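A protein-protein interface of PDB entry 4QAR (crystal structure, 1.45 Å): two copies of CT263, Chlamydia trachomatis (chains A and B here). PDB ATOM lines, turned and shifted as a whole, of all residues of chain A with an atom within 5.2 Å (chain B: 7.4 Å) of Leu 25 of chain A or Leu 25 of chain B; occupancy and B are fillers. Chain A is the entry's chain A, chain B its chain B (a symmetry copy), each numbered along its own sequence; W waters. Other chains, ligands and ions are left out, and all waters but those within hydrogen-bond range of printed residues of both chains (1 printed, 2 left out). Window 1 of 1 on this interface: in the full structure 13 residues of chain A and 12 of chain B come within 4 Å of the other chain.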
ATOM      1  N   ARG A  21      39.338   9.199 -13.974  1.00  0.00           N
ATOM      2  CA  ARG A  21      37.872   9.204 -13.882  1.00  0.00           C
ATOM      3  C   ARG A  21      37.400   9.260 -12.426  1.00  0.00           C
ATOM      4  O   ARG A  21      36.385   9.917 -12.140  1.00  0.00           O
ATOM      5  CB  ARG A  21      37.271   8.023 -14.664  1.00  0.00           C
ATOM      6  CG  ARG A  21      37.527   8.045 -16.158  1.00  0.00           C
ATOM      7  CD  ARG A  21      37.095   9.365 -16.845  1.00  0.00           C
ATOM      8  NE  ARG A  21      35.750   9.738 -16.449  1.00  0.00           N
ATOM      9  CZ  ARG A  21      35.213  10.941 -16.565  1.00  0.00           C
ATOM     10  NH1 ARG A  21      35.816  11.893 -17.261  1.00  0.00           N
ATOM     11  NH2 ARG A  21      34.011  11.129 -16.063  1.00  0.00           N
ATOM     12  N   THR A  22      38.142   8.656 -11.484  1.00  0.00           N
ATOM     13  CA  THR A  22      37.785   8.794 -10.082  1.00  0.00           C
ATOM     14  C   THR A  22      37.928  10.249  -9.628  1.00  0.00           C
ATOM     15  O   THR A  22      37.075  10.775  -8.900  1.00  0.00           O
ATOM     16  CB  THR A  22      38.657   7.859  -9.253  1.00  0.00           C
ATOM     17  OG1 THR A  22      38.309   6.492  -9.529  1.00  0.00           O
ATOM     18  CG2 THR A  22      38.448   8.116  -7.777  1.00  0.00           C
ATOM     19  N   LEU A  23      38.990  10.923 -10.068  1.00  0.00           N
ATOM     20  CA  LEU A  23      39.169  12.330  -9.746  1.00  0.00           C
ATOM     21  C   LEU A  23      38.025  13.192 -10.284  1.00  0.00           C
ATOM     22  O   LEU A  23      37.751  14.252  -9.724  1.00  0.00           O
ATOM     23  CB  LEU A  23      40.531  12.825 -10.198  1.00  0.00           C
ATOM     24  CG  LEU A  23      41.729  12.296  -9.392  1.00  0.00           C
ATOM     25  CD1 LEU A  23      42.998  12.658 -10.124  1.00  0.00           C
ATOM     26  CD2 LEU A  23      41.779  12.803  -7.963  1.00  0.00           C
ATOM     27  N   SER A  24      37.362  12.758 -11.365  1.00  0.00           N
ATOM     28  CA  SER A  24      36.201  13.480 -11.867  1.00  0.00           C
ATOM     29  C   SER A  24      34.940  13.271 -11.031  1.00  0.00           C
ATOM     30  O   SER A  24      34.029  14.110 -11.102  1.00  0.00           O
ATOM     31  CB  SER A  24      35.973  13.121 -13.344  1.00  0.00           C
ATOM     32  OG  SER A  24      35.027  13.994 -13.923  1.00  0.00           O
ATOM     33  N   LEU A  25      34.861  12.207 -10.232  1.00  0.00           N
ATOM     34  CA  LEU A  25      33.600  11.835  -9.571  1.00  0.00           C
ATOM     35  C   LEU A  25      33.230  12.777  -8.451  1.00  0.00           C
ATOM     36  O   LEU A  25      32.044  12.922  -8.136  1.00  0.00           O
ATOM     37  CB  LEU A  25      33.720  10.470  -8.909  1.00  0.00           C
ATOM     38  CG  LEU A  25      33.781   9.238  -9.771  1.00  0.00           C
ATOM     39  CD1 LEU A  25      33.937   8.046  -8.820  1.00  0.00           C
ATOM     40  CD2 LEU A  25      32.525   9.103 -10.602  1.00  0.00           C
ATOM     41  N   PHE A  26      34.224  13.384  -7.811  1.00  0.00           N
ATOM     42  CA  PHE A  26      34.011  14.272  -6.677  1.00  0.00           C
ATOM     43  C   PHE A  26      34.740  15.576  -6.927  1.00  0.00           C
ATOM     44  O   PHE A  26      35.737  15.596  -7.658  1.00  0.00           O
ATOM     45  CB  PHE A  26      34.565  13.652  -5.391  1.00  0.00           C
ATOM     46  CG  PHE A  26      34.013  12.295  -5.107  1.00  0.00           C
ATOM     47  CD1 PHE A  26      32.755  12.163  -4.558  1.00  0.00           C
ATOM     48  CD2 PHE A  26      34.730  11.155  -5.425  1.00  0.00           C
ATOM     49  CE1 PHE A  26      32.208  10.914  -4.300  1.00  0.00           C
ATOM     50  CE2 PHE A  26      34.202   9.892  -5.151  1.00  0.00           C
ATOM     51  CZ  PHE A  26      32.943   9.778  -4.579  1.00  0.00           C
ATOM     52  N   PRO A  27      34.277  16.677  -6.330  1.00  0.00           N
ATOM     53  CA  PRO A  27      34.983  17.968  -6.474  1.00  0.00           C
ATOM     54  C   PRO A  27      36.207  18.068  -5.566  1.00  0.00           C
ATOM     55  O   PRO A  27      36.260  18.819  -4.584  1.00  0.00           O
ATOM     56  CB  PRO A  27      33.885  18.982  -6.133  1.00  0.00           C
ATOM     57  CG  PRO A  27      32.964  18.246  -5.224  1.00  0.00           C
ATOM     58  CD  PRO A  27      32.946  16.836  -5.712  1.00  0.00           C
ATOM     59  N   GLN A 185      37.374   4.598 -16.047  1.00  0.00           N
ATOM     60  CA  GLN A 185      35.963   4.689 -15.712  1.00  0.00           C
ATOM     61  C   GLN A 185      35.480   3.471 -14.933  1.00  0.00           C
ATOM     62  O   GLN A 185      34.673   3.616 -14.009  1.00  0.00           O
ATOM     63  CB  GLN A 185      35.121   4.950 -16.971  1.00  0.00           C
ATOM     64  CG  GLN A 185      33.637   5.152 -16.711  1.00  0.00           C
ATOM     65  CD  GLN A 185      33.338   6.427 -15.989  1.00  0.00           C
ATOM     66  OE1 GLN A 185      34.118   7.378 -16.051  1.00  0.00           O
ATOM     67  NE2 GLN A 185      32.215   6.473 -15.298  1.00  0.00           N
ATOM     68  N   ALA A 188      36.403   3.946 -11.388  1.00  0.00           N
ATOM     69  CA  ALA A 188      35.542   4.927 -10.738  1.00  0.00           C
ATOM     70  C   ALA A 188      34.197   4.318 -10.364  1.00  0.00           C
ATOM     71  O   ALA A 188      33.677   4.557  -9.268  1.00  0.00           O
ATOM     72  CB  ALA A 188      35.369   6.127 -11.662  1.00  0.00           C
ATOM     73  N   GLU A 189      33.610   3.532 -11.269  1.00  0.00           N
ATOM     74  CA  GLU A 189      32.328   2.900 -11.008  1.00  0.00           C
ATOM     75  C   GLU A 189      32.398   1.897  -9.862  1.00  0.00           C
ATOM     76  O   GLU A 189      31.401   1.681  -9.160  1.00  0.00           O
ATOM     77  CB  GLU A 189      31.833   2.278 -12.317  1.00  0.00           C
ATOM     78  CG  GLU A 189      31.465   3.370 -13.329  1.00  0.00           C
ATOM     79  CD  GLU A 189      31.180   2.845 -14.732  1.00  0.00           C
ATOM     80  OE1 GLU A 189      31.342   1.622 -14.967  1.00  0.00           O
ATOM     81  OE2 GLU A 189      30.787   3.665 -15.592  1.00  0.00           O
ATOM     82  N   PHE A 192      32.752   4.001  -6.269  1.00  0.00           N
ATOM     83  CA  PHE A 192      31.615   4.740  -5.713  1.00  0.00           C
ATOM     84  C   PHE A 192      30.803   3.982  -4.667  1.00  0.00           C
ATOM     85  O   PHE A 192      30.548   4.553  -3.599  1.00  0.00           O
ATOM     86  CB  PHE A 192      30.709   5.284  -6.815  1.00  0.00           C
ATOM     87  CG  PHE A 192      29.516   6.000  -6.251  1.00  0.00           C
ATOM     88  CD1 PHE A 192      29.642   7.299  -5.780  1.00  0.00           C
ATOM     89  CD2 PHE A 192      28.300   5.351  -6.100  1.00  0.00           C
ATOM     90  CE1 PHE A 192      28.546   7.960  -5.213  1.00  0.00           C
ATOM     91  CE2 PHE A 192      27.203   6.011  -5.539  1.00  0.00           C
ATOM     92  CZ  PHE A 192      27.337   7.304  -5.094  1.00  0.00           C
ATOM     93  N   LEU B  11      18.312  11.481 -19.179  1.00  0.00           N
ATOM     94  CA  LEU B  11      18.298  12.351 -18.006  1.00  0.00           C
ATOM     95  C   LEU B  11      18.050  13.780 -18.457  1.00  0.00           C
ATOM     96  O   LEU B  11      18.695  14.264 -19.383  1.00  0.00           O
ATOM     97  CB  LEU B  11      19.650  12.318 -17.289  1.00  0.00           C
ATOM     98  CG  LEU B  11      20.324  11.016 -16.889  1.00  0.00           C
ATOM     99  CD1 LEU B  11      21.648  11.325 -16.145  1.00  0.00           C
ATOM    100  CD2 LEU B  11      19.384  10.196 -16.050  1.00  0.00           C
ATOM    101  N   ALA B  19      23.079  20.277 -13.445  1.00  0.00           N
ATOM    102  CA  ALA B  19      23.615  19.146 -14.183  1.00  0.00           C
ATOM    103  C   ALA B  19      25.108  18.922 -13.981  1.00  0.00           C
ATOM    104  O   ALA B  19      25.589  17.818 -14.273  1.00  0.00           O
ATOM    105  CB  ALA B  19      23.387  19.371 -15.682  1.00  0.00           C
ATOM    106  N   ALA B  20      25.839  19.907 -13.453  1.00  0.00           N
ATOM    107  CA  ALA B  20      27.285  19.952 -13.645  1.00  0.00           C
ATOM    108  C   ALA B  20      27.985  18.740 -13.056  1.00  0.00           C
ATOM    109  O   ALA B  20      28.921  18.206 -13.663  1.00  0.00           O
ATOM    110  CB  ALA B  20      27.837  21.225 -13.022  1.00  0.00           C
ATOM    111  N   ARG B  21      27.600  18.312 -11.857  1.00  0.00           N
ATOM    112  CA  ARG B  21      28.315  17.215 -11.224  1.00  0.00           C
ATOM    113  C   ARG B  21      27.935  15.887 -11.872  1.00  0.00           C
ATOM    114  O   ARG B  21      28.790  15.008 -11.973  1.00  0.00           O
ATOM    115  CB  ARG B  21      28.072  17.232  -9.715  1.00  0.00           C
ATOM    116  CG  ARG B  21      28.664  18.443  -8.955  1.00  0.00           C
ATOM    117  CD  ARG B  21      30.153  18.612  -9.190  1.00  0.00           C
ATOM    118  NE  ARG B  21      30.842  17.336  -8.957  1.00  0.00           N
ATOM    119  CZ  ARG B  21      31.982  16.990  -9.510  1.00  0.00           C
ATOM    120  NH1 ARG B  21      32.674  17.839 -10.256  1.00  0.00           N
ATOM    121  NH2 ARG B  21      32.453  15.783  -9.249  1.00  0.00           N
ATOM    122  N   THR B  22      26.686  15.724 -12.333  1.00  0.00           N
ATOM    123  CA  THR B  22      26.317  14.496 -13.043  1.00  0.00           C
ATOM    124  C   THR B  22      27.102  14.369 -14.323  1.00  0.00           C
ATOM    125  O   THR B  22      27.551  13.256 -14.671  1.00  0.00           O
ATOM    126  CB  THR B  22      24.809  14.466 -13.315  1.00  0.00           C
ATOM    127  OG1 THR B  22      24.107  14.331 -12.083  1.00  0.00           O
ATOM    128  CG2 THR B  22      24.409  13.306 -14.234  1.00  0.00           C
ATOM    129  N   LEU B  23      27.341  15.485 -15.008  1.00  0.00           N
ATOM    130  CA  LEU B  23      28.094  15.452 -16.249  1.00  0.00           C
ATOM    131  C   LEU B  23      29.548  15.075 -16.006  1.00  0.00           C
ATOM    132  O   LEU B  23      30.205  14.559 -16.926  1.00  0.00           O
ATOM    133  CB  LEU B  23      27.954  16.796 -16.971  1.00  0.00           C
ATOM    134  CG  LEU B  23      26.554  17.050 -17.570  1.00  0.00           C
ATOM    135  CD1 LEU B  23      26.478  18.505 -18.063  1.00  0.00           C
ATOM    136  CD2 LEU B  23      26.224  16.087 -18.692  1.00  0.00           C
ATOM    137  N   SER B  24      30.066  15.291 -14.793  1.00  0.00           N
ATOM    138  CA  SER B  24      31.419  14.897 -14.424  1.00  0.00           C
ATOM    139  C   SER B  24      31.533  13.387 -14.161  1.00  0.00           C
ATOM    140  O   SER B  24      32.646  12.871 -14.080  1.00  0.00           O
ATOM    141  CB  SER B  24      31.810  15.693 -13.182  1.00  0.00           C
ATOM    142  OG  SER B  24      33.202  15.811 -13.034  1.00  0.00           O
ATOM    143  N   LEU B  25      30.433  12.660 -14.111  1.00  0.00           N
ATOM    144  CA  LEU B  25      30.480  11.255 -13.728  1.00  0.00           C
ATOM    145  C   LEU B  25      30.961  10.353 -14.845  1.00  0.00           C
ATOM    146  O   LEU B  25      31.464   9.276 -14.553  1.00  0.00           O
ATOM    147  CB  LEU B  25      29.096  10.729 -13.352  1.00  0.00           C
ATOM    148  CG  LEU B  25      28.435  11.324 -12.106  1.00  0.00           C
ATOM    149  CD1 LEU B  25      26.958  10.812 -12.034  1.00  0.00           C
ATOM    150  CD2 LEU B  25      29.182  10.948 -10.870  1.00  0.00           C
ATOM    151  N   PHE B  26      30.764  10.739 -16.102  1.00  0.00           N
ATOM    152  CA  PHE B  26      31.074   9.913 -17.256  1.00  0.00           C
ATOM    153  C   PHE B  26      31.751  10.748 -18.324  1.00  0.00           C
ATOM    154  O   PHE B  26      31.515  11.960 -18.410  1.00  0.00           O
ATOM    155  CB  PHE B  26      29.807   9.323 -17.893  1.00  0.00           C
ATOM    156  CG  PHE B  26      28.936   8.539 -16.937  1.00  0.00           C
ATOM    157  CD1 PHE B  26      29.218   7.224 -16.681  1.00  0.00           C
ATOM    158  CD2 PHE B  26      27.876   9.131 -16.288  1.00  0.00           C
ATOM    159  CE1 PHE B  26      28.421   6.471 -15.815  1.00  0.00           C
ATOM    160  CE2 PHE B  26      27.082   8.381 -15.418  1.00  0.00           C
ATOM    161  CZ  PHE B  26      27.384   7.056 -15.181  1.00  0.00           C
ATOM    162  N   PRO B  27      32.542  10.127 -19.176  1.00  0.00           N
ATOM    163  CA  PRO B  27      33.224  10.825 -20.292  1.00  0.00           C
ATOM    164  C   PRO B  27      32.252  10.999 -21.456  1.00  0.00           C
ATOM    165  O   PRO B  27      32.356  10.407 -22.535  1.00  0.00           O
ATOM    166  CB  PRO B  27      34.394   9.886 -20.610  1.00  0.00           C
ATOM    167  CG  PRO B  27      33.887   8.578 -20.294  1.00  0.00           C
ATOM    168  CD  PRO B  27      33.052   8.755 -19.031  1.00  0.00           C
ATOM    169  N   PHE B  28      31.276  11.856 -21.220  1.00  0.00           N
ATOM    170  CA  PHE B  28      30.233  12.134 -22.204  1.00  0.00           C
ATOM    171  C   PHE B  28      30.841  12.782 -23.437  1.00  0.00           C
ATOM    172  O   PHE B  28      31.862  13.466 -23.372  1.00  0.00           O
ATOM    173  CB  PHE B  28      29.239  13.156 -21.639  1.00  0.00           C
ATOM    174  CG  PHE B  28      28.269  12.604 -20.613  1.00  0.00           C
ATOM    175  CD1 PHE B  28      27.181  11.844 -20.993  1.00  0.00           C
ATOM    176  CD2 PHE B  28      28.456  12.859 -19.244  1.00  0.00           C
ATOM    177  CE1 PHE B  28      26.323  11.305 -20.074  1.00  0.00           C
ATOM    178  CE2 PHE B  28      27.581  12.337 -18.338  1.00  0.00           C
ATOM    179  CZ  PHE B  28      26.502  11.588 -18.731  1.00  0.00           C
ATOM    180  N   TYR B  38      26.599   9.138 -23.687  1.00  0.00           N
ATOM    181  CA  TYR B  38      27.590   8.163 -23.244  1.00  0.00           C
ATOM    182  C   TYR B  38      27.030   6.765 -23.410  1.00  0.00           C
ATOM    183  O   TYR B  38      25.860   6.514 -23.104  1.00  0.00           O
ATOM    184  CB  TYR B  38      27.901   8.395 -21.762  1.00  0.00           C
ATOM    185  CG  TYR B  38      28.823   7.390 -21.151  1.00  0.00           C
ATOM    186  CD1 TYR B  38      30.143   7.326 -21.534  1.00  0.00           C
ATOM    187  CD2 TYR B  38      28.374   6.521 -20.162  1.00  0.00           C
ATOM    188  CE1 TYR B  38      31.022   6.341 -20.986  1.00  0.00           C
ATOM    189  CE2 TYR B  38      29.215   5.604 -19.606  1.00  0.00           C
ATOM    190  CZ  TYR B  38      30.524   5.522 -20.006  1.00  0.00           C
ATOM    191  OH  TYR B  38      31.323   4.563 -19.425  1.00  0.00           O
ATOM    192  N   LEU B  45      23.261   6.312 -22.169  1.00  0.00           N
ATOM    193  CA  LEU B  45      22.914   7.362 -21.220  1.00  0.00           C
ATOM    194  C   LEU B  45      23.028   8.705 -21.923  1.00  0.00           C
ATOM    195  O   LEU B  45      24.139   9.165 -22.219  1.00  0.00           O
ATOM    196  CB  LEU B  45      23.853   7.336 -20.020  1.00  0.00           C
ATOM    197  CG  LEU B  45      23.533   8.400 -18.997  1.00  0.00           C
ATOM    198  CD1 LEU B  45      22.132   8.247 -18.487  1.00  0.00           C
ATOM    199  CD2 LEU B  45      24.533   8.291 -17.847  1.00  0.00           C
ATOM    200  N   GLN B 185      26.091  17.729  -6.567  1.00  0.00           N
ATOM    201  CA  GLN B 185      26.752  16.466  -6.254  1.00  0.00           C
ATOM    202  C   GLN B 185      25.770  15.467  -5.651  1.00  0.00           C
ATOM    203  O   GLN B 185      25.849  14.281  -5.946  1.00  0.00           O
ATOM    204  CB  GLN B 185      27.907  16.705  -5.281  1.00  0.00           C
ATOM    205  CG  GLN B 185      28.738  15.436  -4.950  1.00  0.00           C
ATOM    206  CD  GLN B 185      29.565  14.922  -6.113  1.00  0.00           C
ATOM    207  OE1 GLN B 185      29.820  15.628  -7.090  1.00  0.00           O
ATOM    208  NE2 GLN B 185      30.011  13.684  -6.008  1.00  0.00           N
ATOM    209  N   LEU B 187      22.674  15.126  -6.497  1.00  0.00           N
ATOM    210  CA  LEU B 187      21.998  14.543  -7.650  1.00  0.00           C
ATOM    211  C   LEU B 187      22.888  13.520  -8.343  1.00  0.00           C
ATOM    212  O   LEU B 187      22.416  12.444  -8.757  1.00  0.00           O
ATOM    213  CB  LEU B 187      21.565  15.635  -8.639  1.00  0.00           C
ATOM    214  CG  LEU B 187      20.524  16.657  -8.119  1.00  0.00           C
ATOM    215  CD1 LEU B 187      20.244  17.710  -9.103  1.00  0.00           C
ATOM    216  CD2 LEU B 187      19.252  15.933  -7.745  1.00  0.00           C
ATOM    217  N   ALA B 188      24.166  13.860  -8.545  1.00  0.00           N
ATOM    218  CA  ALA B 188      25.091  12.962  -9.226  1.00  0.00           C
ATOM    219  C   ALA B 188      25.222  11.648  -8.475  1.00  0.00           C
ATOM    220  O   ALA B 188      25.264  10.573  -9.095  1.00  0.00           O
ATOM    221  CB  ALA B 188      26.461  13.614  -9.392  1.00  0.00           C
ATOM    222  N   GLU B 189      25.271  11.707  -7.135  1.00  0.00           N
ATOM    223  CA  GLU B 189      25.426  10.500  -6.328  1.00  0.00           C
ATOM    224  C   GLU B 189      24.165   9.645  -6.283  1.00  0.00           C
ATOM    225  O   GLU B 189      24.253   8.430  -6.124  1.00  0.00           O
ATOM    226  CB  GLU B 189      25.865  10.892  -4.924  1.00  0.00           C
ATOM    227  CG  GLU B 189      27.221  11.499  -4.939  1.00  0.00           C
ATOM    228  CD  GLU B 189      27.701  11.996  -3.611  1.00  0.00           C
ATOM    229  OE1 GLU B 189      26.870  12.197  -2.684  1.00  0.00           O
ATOM    230  OE2 GLU B 189      28.923  12.234  -3.526  1.00  0.00           O
ATOM    231  N   ALA B 190      23.009  10.222  -6.544  1.00  0.00           N
ATOM    232  CA  ALA B 190      21.808   9.428  -6.734  1.00  0.00           C
ATOM    233  C   ALA B 190      21.727   8.841  -8.141  1.00  0.00           C
ATOM    234  O   ALA B 190      21.194   7.743  -8.310  1.00  0.00           O
ATOM    235  CB  ALA B 190      20.577  10.281  -6.420  1.00  0.00           C
ATOM    236  N   ILE B 191      22.285   9.513  -9.148  1.00  0.00           N
ATOM    237  CA  ILE B 191      22.211   9.051 -10.535  1.00  0.00           C
ATOM    238  C   ILE B 191      23.224   7.938 -10.812  1.00  0.00           C
ATOM    239  O   ILE B 191      22.957   7.020 -11.594  1.00  0.00           O
ATOM    240  CB  ILE B 191      22.403  10.219 -11.515  1.00  0.00           C
ATOM    241  CG1 ILE B 191      21.119  11.074 -11.517  1.00  0.00           C
ATOM    242  CG2 ILE B 191      22.789   9.742 -12.936  1.00  0.00           C
ATOM    243  CD1 ILE B 191      21.301  12.419 -12.080  1.00  0.00           C
ATOM    244  N   PHE B 192      24.431   8.033 -10.262  1.00  0.00           N
ATOM    245  CA  PHE B 192      25.486   7.085 -10.614  1.00  0.00           C
ATOM    246  C   PHE B 192      25.052   5.637 -10.400  1.00  0.00           C
ATOM    247  O   PHE B 192      25.287   4.818 -11.301  1.00  0.00           O
ATOM    248  CB  PHE B 192      26.767   7.472  -9.849  1.00  0.00           C
ATOM    249  CG  PHE B 192      28.103   6.996 -10.470  1.00  0.00           C
ATOM    250  CD1 PHE B 192      28.433   7.249 -11.794  1.00  0.00           C
ATOM    251  CD2 PHE B 192      29.062   6.363  -9.673  1.00  0.00           C
ATOM    252  CE1 PHE B 192      29.651   6.855 -12.316  1.00  0.00           C
ATOM    253  CE2 PHE B 192      30.283   5.988 -10.190  1.00  0.00           C
ATOM    254  CZ  PHE B 192      30.574   6.228 -11.514  1.00  0.00           C
ATOM    255  N   PRO B 193      24.406   5.258  -9.292  1.00  0.00           N
ATOM    256  CA  PRO B 193      23.982   3.862  -9.148  1.00  0.00           C
ATOM    257  C   PRO B 193      22.852   3.453 -10.082  1.00  0.00           C
ATOM    258  O   PRO B 193      22.791   2.272 -10.447  1.00  0.00           O
ATOM    259  CB  PRO B 193      23.602   3.736  -7.665  1.00  0.00           C
ATOM    260  CG  PRO B 193      23.501   5.095  -7.148  1.00  0.00           C
ATOM    261  CD  PRO B 193      24.191   6.047  -8.069  1.00  0.00           C
ATOM    262  N   TYR B 195      22.558   4.242 -13.236  1.00  0.00           N
ATOM    263  CA  TYR B 195      23.288   3.779 -14.401  1.00  0.00           C
ATOM    264  C   TYR B 195      23.774   2.345 -14.204  1.00  0.00           C
ATOM    265  O   TYR B 195      23.594   1.476 -15.076  1.00  0.00           O
ATOM    266  CB  TYR B 195      24.451   4.735 -14.663  1.00  0.00           C
ATOM    267  CG  TYR B 195      25.340   4.258 -15.760  1.00  0.00           C
ATOM    268  CD1 TYR B 195      25.011   4.472 -17.100  1.00  0.00           C
ATOM    269  CD2 TYR B 195      26.495   3.560 -15.477  1.00  0.00           C
ATOM    270  CE1 TYR B 195      25.816   4.033 -18.108  1.00  0.00           C
ATOM    271  CE2 TYR B 195      27.305   3.117 -16.478  1.00  0.00           C
ATOM    272  CZ  TYR B 195      26.954   3.344 -17.799  1.00  0.00           C
ATOM    273  OH  TYR B 195      27.761   2.901 -18.803  1.00  0.00           O
HETATM  274  O   HOH W   1      30.343   3.006 -17.869  1.00  0.00           O
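O of Leu 25 of chain B sits at hydrogen-bond distance from NE2 of Gln 185 of chain A (3.0 Å).
The guanidinium group (NH2) of Arg 21 of chain A lies close to the backbone NH (N) of Phe 26 of chain B (3.3 Å).
The guanidinium group (NH2) of Arg 21 of chain B sits close to the backbone NH (N) of Phe 26 of chain A, at 3.3 Å.
The guanidinium group of Arg 21 of chain A sits close to the backbone carbonyl oxygen of Leu 25 of chain B (3.5 Å).
The backbone carbonyl oxygen (O) of Ser 24 of chain A lies within hydrogen-bond range of the guanidinium group (NH2) of Arg 21 of chain B, 3.0 Å away.
The side-chain hydroxyl of Ser 24 of chain A lies within hydrogen-bond range of the backbone carbonyl oxygen of Ser 24 of chain B, 2.6 Å away.
The side-chain amide nitrogen of Gln 185 of chain B lies within hydrogen-bond range of the backbone carbonyl oxygen of Leu 25 of chain A, 3.0 Å away.
NH2 of Arg 21 of chain B is in hydrogen-bond range of O of Leu 25 of chain A (3.1 Å).
The guanidinium group (NH2) of Arg 21 of chain A is in hydrogen-bond range of the backbone carbonyl oxygen (O) of Ser 24 of chain B (3.0 Å).
OE2 of Glu 189 of chain A is in hydrogen-bond range of NE2 of Gln 185 of chain A (3.2 Å).
N of Leu 45 of chain B sits at hydrogen-bond distance from O of Tyr 38 of chain B (2.8 Å).
The guanidinium group of Arg 21 of chain A lies within hydrogen-bond range of the side-chain amide oxygen of Gln 185 of chain A (2.9 Å).
OG of Ser 24 of chain B sits at hydrogen-bond distance from NH1 of Arg 21 of chain B.
OE1 of Gln 185 of chain B is in hydrogen-bond range of NE of Arg 21 of chain B, 2.7 Å away.
NE2 of Gln 185 of chain B is in hydrogen-bond range of OE2 of Glu 189 of chain B (3.1 Å).
Among the printed residues, merely in contact across the chains: Gln 185 of chain A with Phe 26 of chain B (3.4 Å), Phe 192 of chain A with Glu 189 of chain B (3.4 Å), Gln 185 of chain A with Pro 27 of chain B (3.5 Å), Phe 26 of chain A with Gln 185 of chain B (3.5 Å), Phe 192 of chain A with Phe 192 of chain B (3.5 Å), Glu 189 of chain A with Phe 192 of chain B (3.5 Å), Pro 27 of chain A with Arg 21 of chain B (3.6 Å), Arg 21 of chain A with Pro 27 of chain B (3.6 Å), Leu 25 of chain A with Phe 192 of chain B (3.6 Å), Gln 185 of chain A with Tyr 38 of chain B (3.6 Å), Pro 27 of chain A with Gln 185 of chain B (3.6 Å), Phe 26 of chain A with Glu 189 of chain B (3.6 Å), Glu 189 of chain A with Tyr 195 of chain B (3.6 Å), Glu 189 of chain A with Phe 26 of chain B (3.7 Å), Ala 188 of chain A with Phe 192 of chain B (3.8 Å), Leu 25 of chain A with Leu 25 of chain B (3.8 Å), Phe 192 of chain A with Pro 193 of chain B (3.9 Å), Gln 185 of chain A with Phe 192 of chain B (3.95 Å) and Glu 189 of chain A with Tyr 38 of chain B (3.97 Å).
Of the printed residues of chain B, Ser 24 of chain A touches Arg 21 (3.0 Å) and Ser 24 (2.6 Å).
Of chain B, only Arg 21 (3.1 Å), Leu 25 (3.8 Å), Gln 185 (3.0 Å) and Phe 192 (3.6 Å) come within 4 Å of Leu 25 of chain A.
Of the printed residues of chain B, Glu 189 of chain A touches Phe 26 (3.7 Å), Tyr 38 (3.97 Å), Phe 192 (3.5 Å) and Tyr 195 (3.6 Å).
Leu 25 of chain B touches just these residues of chain A: Arg 21, Leu 25 and Gln 185.
Printed residues of chain A within 4 Å of Phe 26 of chain B: Arg 21, Gln 185 and Glu 189.
Phe 28 of chain B touches none of the printed residues of chain A.
Of the printed residues of chain A, Gln 185 of chain B touches Leu 25 (3.0 Å), Phe 26 (3.5 Å) and Pro 27 (3.6 Å).
The nearest residue of chain A that does not touch Leu 25 of chain B is Ser 24 of chain A (4.8 Å).
The nearest printed residue of chain B that does not touch Ser 24 of chain A is Leu 25 of chain B (4.8 Å).
Of the 11 printed residues of chain A, 9 touch a printed residue of chain B.
Hydrophobic or aromatic side chains of chain B that line the printed part of chain A: Leu 25, Phe 26, Pro 27, Tyr 38, Phe 192, Pro 193 and Tyr 195.
Among the printed residues, 28 pairs touch across the chains.
Among the printed residues, no Asp or Glu carboxylate lies within 4 Å of a Lys or Arg side-chain nitrogen of the other chain.
Leu 25 of chain A touches Gln 185 of chain B, and with the chains exchanged Gln 185 of chain A touches Leu 25 of chain B.
Phe 26 of chain A touches Gln 185 of chain B, and with the chains exchanged Gln 185 of chain A touches Phe 26 of chain B.
Phe 26 of chain A touches Glu 189 of chain B, and with the chains exchanged Glu 189 of chain A touches Phe 26 of chain B.
Phe 192 of chain A touches its own counterpart, Phe 192 of chain B.
Positions printed for both chains: 21, 22, 23, 24, 25, 26, 27, 185, 188, 189 and 192.
Of the 28 pairs that touch across the chains among the printed residues, 21 have their exchanged pair printed and touching as well.
Water W1 lies within hydrogen-bond range of the side-chain hydroxyl (OH) of Tyr 38 of chain B (2.4 Å), the side-chain carboxylate (OE2) of Glu 189 of chain A (2.4 Å) and the side-chain hydroxyl (OH) of Tyr 195 of chain B (2.7 Å).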
